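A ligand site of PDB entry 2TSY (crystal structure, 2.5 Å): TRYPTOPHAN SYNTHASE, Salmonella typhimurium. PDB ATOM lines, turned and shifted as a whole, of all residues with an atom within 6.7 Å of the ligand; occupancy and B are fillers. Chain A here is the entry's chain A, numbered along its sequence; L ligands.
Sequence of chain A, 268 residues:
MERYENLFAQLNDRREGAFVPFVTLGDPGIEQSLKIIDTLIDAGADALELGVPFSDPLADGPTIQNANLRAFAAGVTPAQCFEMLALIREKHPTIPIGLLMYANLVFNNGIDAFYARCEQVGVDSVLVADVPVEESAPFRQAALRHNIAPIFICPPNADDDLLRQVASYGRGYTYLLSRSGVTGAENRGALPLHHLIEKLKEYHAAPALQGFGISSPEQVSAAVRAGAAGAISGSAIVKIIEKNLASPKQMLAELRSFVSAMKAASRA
The backbone NH of Ser 235 lies within hydrogen-bond range of an oxygen (O6) of the ligand (3.1 Å). O6 of the ligand is in hydrogen-bond range of OG of Ser 235 (2.7 Å). An oxygen (O1) of the ligand sits at hydrogen-bond distance from the side-chain hydroxyl (OH) of Tyr 175 (2.9 Å). The backbone NH (N) of Gly 213 lies within hydrogen-bond range of an oxygen (O5) of the ligand (2.9 Å). The backbone NH of Gly 234 is in hydrogen-bond range of an oxygen (O4) of the ligand, at 3.1 Å.
O of Gly 184 sits close to O6 of the ligand. Phe 22 touches the ligand. Thr 183 touches the ligand (CG2 to C3, 3.3 Å). O of Gly 211 touches O4 of the ligand (3.8 Å). Phe 212 touches the ligand (CA to O5, 3.2 Å). CG2 of Ile 232 touches O2 of the ligand (3.9 Å). Ser 233 touches the ligand (CA to O4, 3.9 Å).
The backbone NH (N) of Phe 212 sits at hydrogen-bond distance from the side-chain hydroxyl (OG) of Ser 178, 2.5 Å away. The side-chain hydroxyl (OG1) of Thr 183 lies within hydrogen-bond range of the side-chain carboxylate (OD1) of Asp 60. The backbone NH (N) of Phe 22 lies within hydrogen-bond range of the backbone carbonyl oxygen (O) of Ser 233 (2.8 Å). The backbone carbonyl oxygen (O) of Gly 184 is in hydrogen-bond range of the guanidinium group (NH2) of Arg 179, 2.9 Å away. The side-chain hydroxyl of Ser 233 is in hydrogen-bond range of the backbone carbonyl oxygen of Ile 214, at 3.1 Å. The backbone carbonyl oxygen of Val 20 is in hydrogen-bond range of the backbone NH of Ser 233 (3.3 Å).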
ATOM      1  N   VAL A  20     -20.568  -3.238  14.708  1.00  0.00           N
ATOM      2  CA  VAL A  20     -20.005  -3.079  16.035  1.00  0.00           C
ATOM      3  C   VAL A  20     -19.179  -1.769  16.152  1.00  0.00           C
ATOM      4  O   VAL A  20     -18.043  -1.668  15.677  1.00  0.00           O
ATOM      5  CB  VAL A  20     -19.132  -4.331  16.258  1.00  0.00           C
ATOM      6  CG1 VAL A  20     -18.825  -4.369  17.720  1.00  0.00           C
ATOM      7  CG2 VAL A  20     -19.802  -5.633  15.839  1.00  0.00           C
ATOM      8  N   PRO A  21     -19.706  -0.707  16.752  1.00  0.00           N
ATOM      9  CA  PRO A  21     -18.952   0.458  17.169  1.00  0.00           C
ATOM     10  C   PRO A  21     -17.922   0.263  18.281  1.00  0.00           C
ATOM     11  O   PRO A  21     -17.995  -0.668  19.096  1.00  0.00           O
ATOM     12  CB  PRO A  21     -20.014   1.452  17.544  1.00  0.00           C
ATOM     13  CG  PRO A  21     -21.199   1.051  16.709  1.00  0.00           C
ATOM     14  CD  PRO A  21     -21.135  -0.454  16.883  1.00  0.00           C
ATOM     15  N   PHE A  22     -16.966   1.208  18.315  1.00  0.00           N
ATOM     16  CA  PHE A  22     -15.997   1.283  19.389  1.00  0.00           C
ATOM     17  C   PHE A  22     -15.978   2.695  19.960  1.00  0.00           C
ATOM     18  O   PHE A  22     -16.098   3.705  19.252  1.00  0.00           O
ATOM     19  CB  PHE A  22     -14.608   0.917  18.878  1.00  0.00           C
ATOM     20  CG  PHE A  22     -13.562   0.874  19.986  1.00  0.00           C
ATOM     21  CD1 PHE A  22     -12.873   2.046  20.376  1.00  0.00           C
ATOM     22  CD2 PHE A  22     -13.343  -0.344  20.654  1.00  0.00           C
ATOM     23  CE1 PHE A  22     -11.972   1.985  21.437  1.00  0.00           C
ATOM     24  CE2 PHE A  22     -12.431  -0.388  21.703  1.00  0.00           C
ATOM     25  CZ  PHE A  22     -11.749   0.769  22.096  1.00  0.00           C
ATOM     26  N   VAL A  23     -15.903   2.739  21.309  1.00  0.00           N
ATOM     27  CA  VAL A  23     -15.753   3.946  22.104  1.00  0.00           C
ATOM     28  C   VAL A  23     -14.941   3.602  23.372  1.00  0.00           C
ATOM     29  O   VAL A  23     -14.916   2.444  23.824  1.00  0.00           O
ATOM     30  CB  VAL A  23     -17.190   4.509  22.415  1.00  0.00           C
ATOM     31  CG1 VAL A  23     -17.296   5.432  23.601  1.00  0.00           C
ATOM     32  CG2 VAL A  23     -17.492   5.508  21.328  1.00  0.00           C
ATOM     33  N   GLU A  49     -18.105  -2.707  21.223  1.00  0.00           N
ATOM     34  CA  GLU A  49     -16.698  -2.890  21.612  1.00  0.00           C
ATOM     35  C   GLU A  49     -16.391  -1.669  22.481  1.00  0.00           C
ATOM     36  O   GLU A  49     -16.602  -0.509  22.071  1.00  0.00           O
ATOM     37  CB  GLU A  49     -15.719  -2.861  20.457  1.00  0.00           C
ATOM     38  CG  GLU A  49     -15.489  -4.188  19.807  1.00  0.00           C
ATOM     39  CD  GLU A  49     -14.701  -5.152  20.654  1.00  0.00           C
ATOM     40  OE1 GLU A  49     -13.562  -5.462  20.276  1.00  0.00           O
ATOM     41  OE2 GLU A  49     -15.199  -5.621  21.678  1.00  0.00           O
ATOM     42  N   ASP A  60      -2.287   1.110  19.890  1.00  0.00           N
ATOM     43  CA  ASP A  60      -3.197   2.131  19.503  1.00  0.00           C
ATOM     44  C   ASP A  60      -2.517   3.305  18.904  1.00  0.00           C
ATOM     45  O   ASP A  60      -1.498   3.786  19.373  1.00  0.00           O
ATOM     46  CB  ASP A  60      -4.004   2.631  20.674  1.00  0.00           C
ATOM     47  CG  ASP A  60      -5.172   1.735  21.083  1.00  0.00           C
ATOM     48  OD1 ASP A  60      -6.140   1.644  20.321  1.00  0.00           O
ATOM     49  OD2 ASP A  60      -5.139   1.147  22.159  1.00  0.00           O
ATOM     50  N   THR A  63      -5.726   8.785  17.813  1.00  0.00           N
ATOM     51  CA  THR A  63      -7.102   9.137  18.189  1.00  0.00           C
ATOM     52  C   THR A  63      -7.514   8.456  19.495  1.00  0.00           C
ATOM     53  O   THR A  63      -8.039   9.090  20.422  1.00  0.00           O
ATOM     54  CB  THR A  63      -8.101   8.703  17.087  1.00  0.00           C
ATOM     55  OG1 THR A  63      -7.430   8.650  15.805  1.00  0.00           O
ATOM     56  CG2 THR A  63      -9.270   9.674  17.080  1.00  0.00           C
ATOM     57  N   ILE A  64      -7.211   7.148  19.561  1.00  0.00           N
ATOM     58  CA  ILE A  64      -7.540   6.357  20.735  1.00  0.00           C
ATOM     59  C   ILE A  64      -6.615   6.851  21.834  1.00  0.00           C
ATOM     60  O   ILE A  64      -7.152   7.132  22.913  1.00  0.00           O
ATOM     61  CB  ILE A  64      -7.327   4.835  20.495  1.00  0.00           C
ATOM     62  CG1 ILE A  64      -8.062   4.296  19.285  1.00  0.00           C
ATOM     63  CG2 ILE A  64      -7.856   4.119  21.726  1.00  0.00           C
ATOM     64  CD1 ILE A  64      -9.591   4.288  19.387  1.00  0.00           C
ATOM     65  N   LEU A 100     -12.417  -4.485  25.364  1.00  0.00           N
ATOM     66  CA  LEU A 100     -11.105  -4.543  24.739  1.00  0.00           C
ATOM     67  C   LEU A 100     -10.142  -3.930  25.765  1.00  0.00           C
ATOM     68  O   LEU A 100     -10.215  -2.759  26.145  1.00  0.00           O
ATOM     69  CB  LEU A 100     -11.130  -3.745  23.467  1.00  0.00           C
ATOM     70  CG  LEU A 100     -10.007  -3.853  22.449  1.00  0.00           C
ATOM     71  CD1 LEU A 100      -9.351  -2.503  22.333  1.00  0.00           C
ATOM     72  CD2 LEU A 100      -8.979  -4.894  22.837  1.00  0.00           C
ATOM     73  N   LEU A 127     -11.482  -9.183  25.043  1.00  0.00           N
ATOM     74  CA  LEU A 127     -10.360  -9.234  24.098  1.00  0.00           C
ATOM     75  C   LEU A 127      -9.152  -8.688  24.839  1.00  0.00           C
ATOM     76  O   LEU A 127      -9.147  -7.479  25.163  1.00  0.00           O
ATOM     77  CB  LEU A 127     -10.526  -8.279  22.900  1.00  0.00           C
ATOM     78  CG  LEU A 127     -10.132  -8.619  21.469  1.00  0.00           C
ATOM     79  CD1 LEU A 127     -10.336  -7.364  20.614  1.00  0.00           C
ATOM     80  CD2 LEU A 127      -8.717  -9.141  21.410  1.00  0.00           C
ATOM     81  N   TYR A 175     -11.753 -12.163  15.822  1.00  0.00           N
ATOM     82  CA  TYR A 175     -11.397 -10.794  15.466  1.00  0.00           C
ATOM     83  C   TYR A 175     -10.426 -10.982  14.323  1.00  0.00           C
ATOM     84  O   TYR A 175      -9.370 -11.589  14.477  1.00  0.00           O
ATOM     85  CB  TYR A 175     -10.714 -10.063  16.595  1.00  0.00           C
ATOM     86  CG  TYR A 175     -10.677  -8.564  16.327  1.00  0.00           C
ATOM     87  CD1 TYR A 175      -9.788  -8.018  15.387  1.00  0.00           C
ATOM     88  CD2 TYR A 175     -11.534  -7.732  17.041  1.00  0.00           C
ATOM     89  CE1 TYR A 175      -9.759  -6.642  15.147  1.00  0.00           C
ATOM     90  CE2 TYR A 175     -11.498  -6.352  16.806  1.00  0.00           C
ATOM     91  CZ  TYR A 175     -10.618  -5.824  15.856  1.00  0.00           C
ATOM     92  OH  TYR A 175     -10.642  -4.457  15.602  1.00  0.00           O
ATOM     93  N   SER A 178      -7.547  -6.564   9.513  1.00  0.00           N
ATOM     94  CA  SER A 178      -7.487  -5.913   8.247  1.00  0.00           C
ATOM     95  C   SER A 178      -6.049  -5.708   7.801  1.00  0.00           C
ATOM     96  O   SER A 178      -5.654  -6.053   6.674  1.00  0.00           O
ATOM     97  CB  SER A 178      -8.179  -4.580   8.377  1.00  0.00           C
ATOM     98  OG  SER A 178      -8.905  -4.512   9.605  1.00  0.00           O
ATOM     99  N   ARG A 179      -5.177  -5.184   8.659  1.00  0.00           N
ATOM    100  CA  ARG A 179      -3.832  -4.813   8.243  1.00  0.00           C
ATOM    101  C   ARG A 179      -2.880  -5.022   9.408  1.00  0.00           C
ATOM    102  O   ARG A 179      -3.286  -5.470  10.478  1.00  0.00           O
ATOM    103  CB  ARG A 179      -3.861  -3.352   7.799  1.00  0.00           C
ATOM    104  CG  ARG A 179      -4.624  -2.454   8.744  1.00  0.00           C
ATOM    105  CD  ARG A 179      -4.518  -1.015   8.297  1.00  0.00           C
ATOM    106  NE  ARG A 179      -5.109  -0.046   9.237  1.00  0.00           N
ATOM    107  CZ  ARG A 179      -4.611   0.204  10.472  1.00  0.00           C
ATOM    108  NH1 ARG A 179      -3.517  -0.422  10.988  1.00  0.00           N
ATOM    109  NH2 ARG A 179      -5.204   1.164  11.170  1.00  0.00           N
ATOM    110  N   VAL A 182      -1.271  -0.314  14.088  1.00  0.00           N
ATOM    111  CA  VAL A 182      -1.963  -0.037  15.335  1.00  0.00           C
ATOM    112  C   VAL A 182      -3.284   0.611  14.929  1.00  0.00           C
ATOM    113  O   VAL A 182      -3.414   1.047  13.776  1.00  0.00           O
ATOM    114  CB  VAL A 182      -1.124   0.924  16.285  1.00  0.00           C
ATOM    115  CG1 VAL A 182       0.107   0.171  16.768  1.00  0.00           C
ATOM    116  CG2 VAL A 182      -0.706   2.220  15.582  1.00  0.00           C
ATOM    117  N   THR A 183      -4.269   0.725  15.805  1.00  0.00           N
ATOM    118  CA  THR A 183      -5.568   1.210  15.417  1.00  0.00           C
ATOM    119  C   THR A 183      -5.509   2.611  14.825  1.00  0.00           C
ATOM    120  O   THR A 183      -5.117   3.570  15.496  1.00  0.00           O
ATOM    121  CB  THR A 183      -6.509   1.156  16.661  1.00  0.00           C
ATOM    122  OG1 THR A 183      -6.027   2.083  17.623  1.00  0.00           O
ATOM    123  CG2 THR A 183      -6.566  -0.233  17.280  1.00  0.00           C
ATOM    124  N   GLY A 184      -5.819   2.773  13.546  1.00  0.00           N
ATOM    125  CA  GLY A 184      -5.825   4.087  12.933  1.00  0.00           C
ATOM    126  C   GLY A 184      -6.950   4.151  11.909  1.00  0.00           C
ATOM    127  O   GLY A 184      -7.311   3.138  11.327  1.00  0.00           O
ATOM    128  N   ALA A 185      -7.529   5.326  11.669  1.00  0.00           N
ATOM    129  CA  ALA A 185      -8.611   5.463  10.697  1.00  0.00           C
ATOM    130  C   ALA A 185      -8.117   5.491   9.237  1.00  0.00           C
ATOM    131  O   ALA A 185      -8.825   6.022   8.365  1.00  0.00           O
ATOM    132  CB  ALA A 185      -9.374   6.749  10.986  1.00  0.00           C
ATOM    133  N   GLU A 186      -6.925   4.941   8.924  1.00  0.00           N
ATOM    134  CA  GLU A 186      -6.365   5.102   7.589  1.00  0.00           C
ATOM    135  C   GLU A 186      -5.488   4.022   6.980  1.00  0.00           C
ATOM    136  O   GLU A 186      -4.507   3.490   7.519  1.00  0.00           O
ATOM    137  CB  GLU A 186      -5.602   6.459   7.488  1.00  0.00           C
ATOM    138  CG  GLU A 186      -4.726   6.969   8.649  1.00  0.00           C
ATOM    139  CD  GLU A 186      -5.417   7.706   9.805  1.00  0.00           C
ATOM    140  OE1 GLU A 186      -4.962   7.555  10.948  1.00  0.00           O
ATOM    141  OE2 GLU A 186      -6.397   8.433   9.584  1.00  0.00           O
ATOM    142  N   GLY A 211     -11.572  -5.977  11.446  1.00  0.00           N
ATOM    143  CA  GLY A 211     -11.191  -4.947  12.383  1.00  0.00           C
ATOM    144  C   GLY A 211     -10.558  -3.607  12.038  1.00  0.00           C
ATOM    145  O   GLY A 211     -11.237  -2.589  11.900  1.00  0.00           O
ATOM    146  N   PHE A 212      -9.231  -3.500  11.910  1.00  0.00           N
ATOM    147  CA  PHE A 212      -8.622  -2.180  11.877  1.00  0.00           C
ATOM    148  C   PHE A 212      -8.843  -1.305  10.654  1.00  0.00           C
ATOM    149  O   PHE A 212      -8.764  -1.788   9.528  1.00  0.00           O
ATOM    150  CB  PHE A 212      -7.101  -2.301  12.108  1.00  0.00           C
ATOM    151  CG  PHE A 212      -6.608  -2.646  13.528  1.00  0.00           C
ATOM    152  CD1 PHE A 212      -7.471  -3.095  14.543  1.00  0.00           C
ATOM    153  CD2 PHE A 212      -5.234  -2.541  13.794  1.00  0.00           C
ATOM    154  CE1 PHE A 212      -6.954  -3.445  15.802  1.00  0.00           C
ATOM    155  CE2 PHE A 212      -4.739  -2.882  15.057  1.00  0.00           C
ATOM    156  CZ  PHE A 212      -5.596  -3.338  16.050  1.00  0.00           C
ATOM    157  N   GLY A 213      -9.278  -0.060  10.839  1.00  0.00           N
ATOM    158  CA  GLY A 213      -9.261   0.924   9.765  1.00  0.00           C
ATOM    159  C   GLY A 213     -10.495   1.047   8.881  1.00  0.00           C
ATOM    160  O   GLY A 213     -10.387   1.313   7.681  1.00  0.00           O
ATOM    161  N   ILE A 214     -11.714   0.858   9.406  1.00  0.00           N
ATOM    162  CA  ILE A 214     -12.906   1.028   8.599  1.00  0.00           C
ATOM    163  C   ILE A 214     -13.474   2.350   9.030  1.00  0.00           C
ATOM    164  O   ILE A 214     -13.576   2.688  10.206  1.00  0.00           O
ATOM    165  CB  ILE A 214     -13.827  -0.183   8.877  1.00  0.00           C
ATOM    166  CG1 ILE A 214     -13.223  -1.372   8.172  1.00  0.00           C
ATOM    167  CG2 ILE A 214     -15.235   0.025   8.359  1.00  0.00           C
ATOM    168  CD1 ILE A 214     -13.355  -2.600   9.010  1.00  0.00           C
ATOM    169  N   SER A 215     -13.754   3.138   8.028  1.00  0.00           N
ATOM    170  CA  SER A 215     -14.280   4.479   8.223  1.00  0.00           C
ATOM    171  C   SER A 215     -15.334   4.881   7.182  1.00  0.00           C
ATOM    172  O   SER A 215     -16.090   5.857   7.316  1.00  0.00           O
ATOM    173  CB  SER A 215     -13.090   5.441   8.184  1.00  0.00           C
ATOM    174  OG  SER A 215     -11.885   4.772   7.774  1.00  0.00           O
ATOM    175  N   ILE A 232     -15.687  -3.898  12.385  1.00  0.00           N
ATOM    176  CA  ILE A 232     -15.606  -3.154  13.637  1.00  0.00           C
ATOM    177  C   ILE A 232     -15.031  -1.801  13.224  1.00  0.00           C
ATOM    178  O   ILE A 232     -14.136  -1.678  12.389  1.00  0.00           O
ATOM    179  CB  ILE A 232     -14.672  -3.878  14.676  1.00  0.00           C
ATOM    180  CG1 ILE A 232     -15.147  -5.329  14.877  1.00  0.00           C
ATOM    181  CG2 ILE A 232     -14.719  -3.144  16.015  1.00  0.00           C
ATOM    182  CD1 ILE A 232     -14.716  -6.086  16.137  1.00  0.00           C
ATOM    183  N   SER A 233     -15.588  -0.733  13.756  1.00  0.00           N
ATOM    184  CA  SER A 233     -15.043   0.575  13.499  1.00  0.00           C
ATOM    185  C   SER A 233     -14.931   1.265  14.861  1.00  0.00           C
ATOM    186  O   SER A 233     -15.848   1.269  15.713  1.00  0.00           O
ATOM    187  CB  SER A 233     -15.967   1.338  12.555  1.00  0.00           C
ATOM    188  OG  SER A 233     -15.697   2.743  12.453  1.00  0.00           O
ATOM    189  N   GLY A 234     -13.708   1.797  14.994  1.00  0.00           N
ATOM    190  CA  GLY A 234     -13.247   2.484  16.182  1.00  0.00           C
ATOM    191  C   GLY A 234     -12.829   3.935  15.989  1.00  0.00           C
ATOM    192  O   GLY A 234     -13.657   4.854  16.165  1.00  0.00           O
ATOM    193  N   SER A 235     -11.556   4.190  15.610  1.00  0.00           N
ATOM    194  CA  SER A 235     -11.059   5.559  15.496  1.00  0.00           C
ATOM    195  C   SER A 235     -12.013   6.464  14.762  1.00  0.00           C
ATOM    196  O   SER A 235     -12.375   7.489  15.322  1.00  0.00           O
ATOM    197  CB  SER A 235      -9.704   5.589  14.803  1.00  0.00           C
ATOM    198  OG  SER A 235      -8.801   4.735  15.485  1.00  0.00           O
ATOM    199  N   ALA A 236     -12.562   5.993  13.632  1.00  0.00           N
ATOM    200  CA  ALA A 236     -13.507   6.775  12.854  1.00  0.00           C
ATOM    201  C   ALA A 236     -14.561   7.495  13.674  1.00  0.00           C
ATOM    202  O   ALA A 236     -14.848   8.674  13.452  1.00  0.00           O
ATOM    203  CB  ALA A 236     -14.223   5.879  11.899  1.00  0.00           C
HETATM  204  O1  LIG L   1     -10.826  -3.054  18.107  1.00  0.00           O
HETATM  205  C1  LIG L   1     -10.566  -1.582  18.508  1.00  0.00           C
HETATM  206  C2  LIG L   1     -10.568  -0.651  17.751  1.00  0.00           C
HETATM  207  O2  LIG L   1     -12.070  -0.695  17.502  1.00  0.00           O
HETATM  208  C3  LIG L   1      -9.711  -0.518  16.414  1.00  0.00           C
HETATM  209  O3  LIG L   1      -9.951   1.027  15.822  1.00  0.00           O
HETATM  210  O4  LIG L   1     -11.171   0.892  13.485  1.00  0.00           O
HETATM  211  O5  LIG L   1      -8.526   0.541  13.603  1.00  0.00           O
HETATM  212  O6  LIG L   1      -9.487   2.586  13.959  1.00  0.00           O
HETATM  213  P1  LIG L   1      -9.838   1.281  14.179  1.00  0.00           P
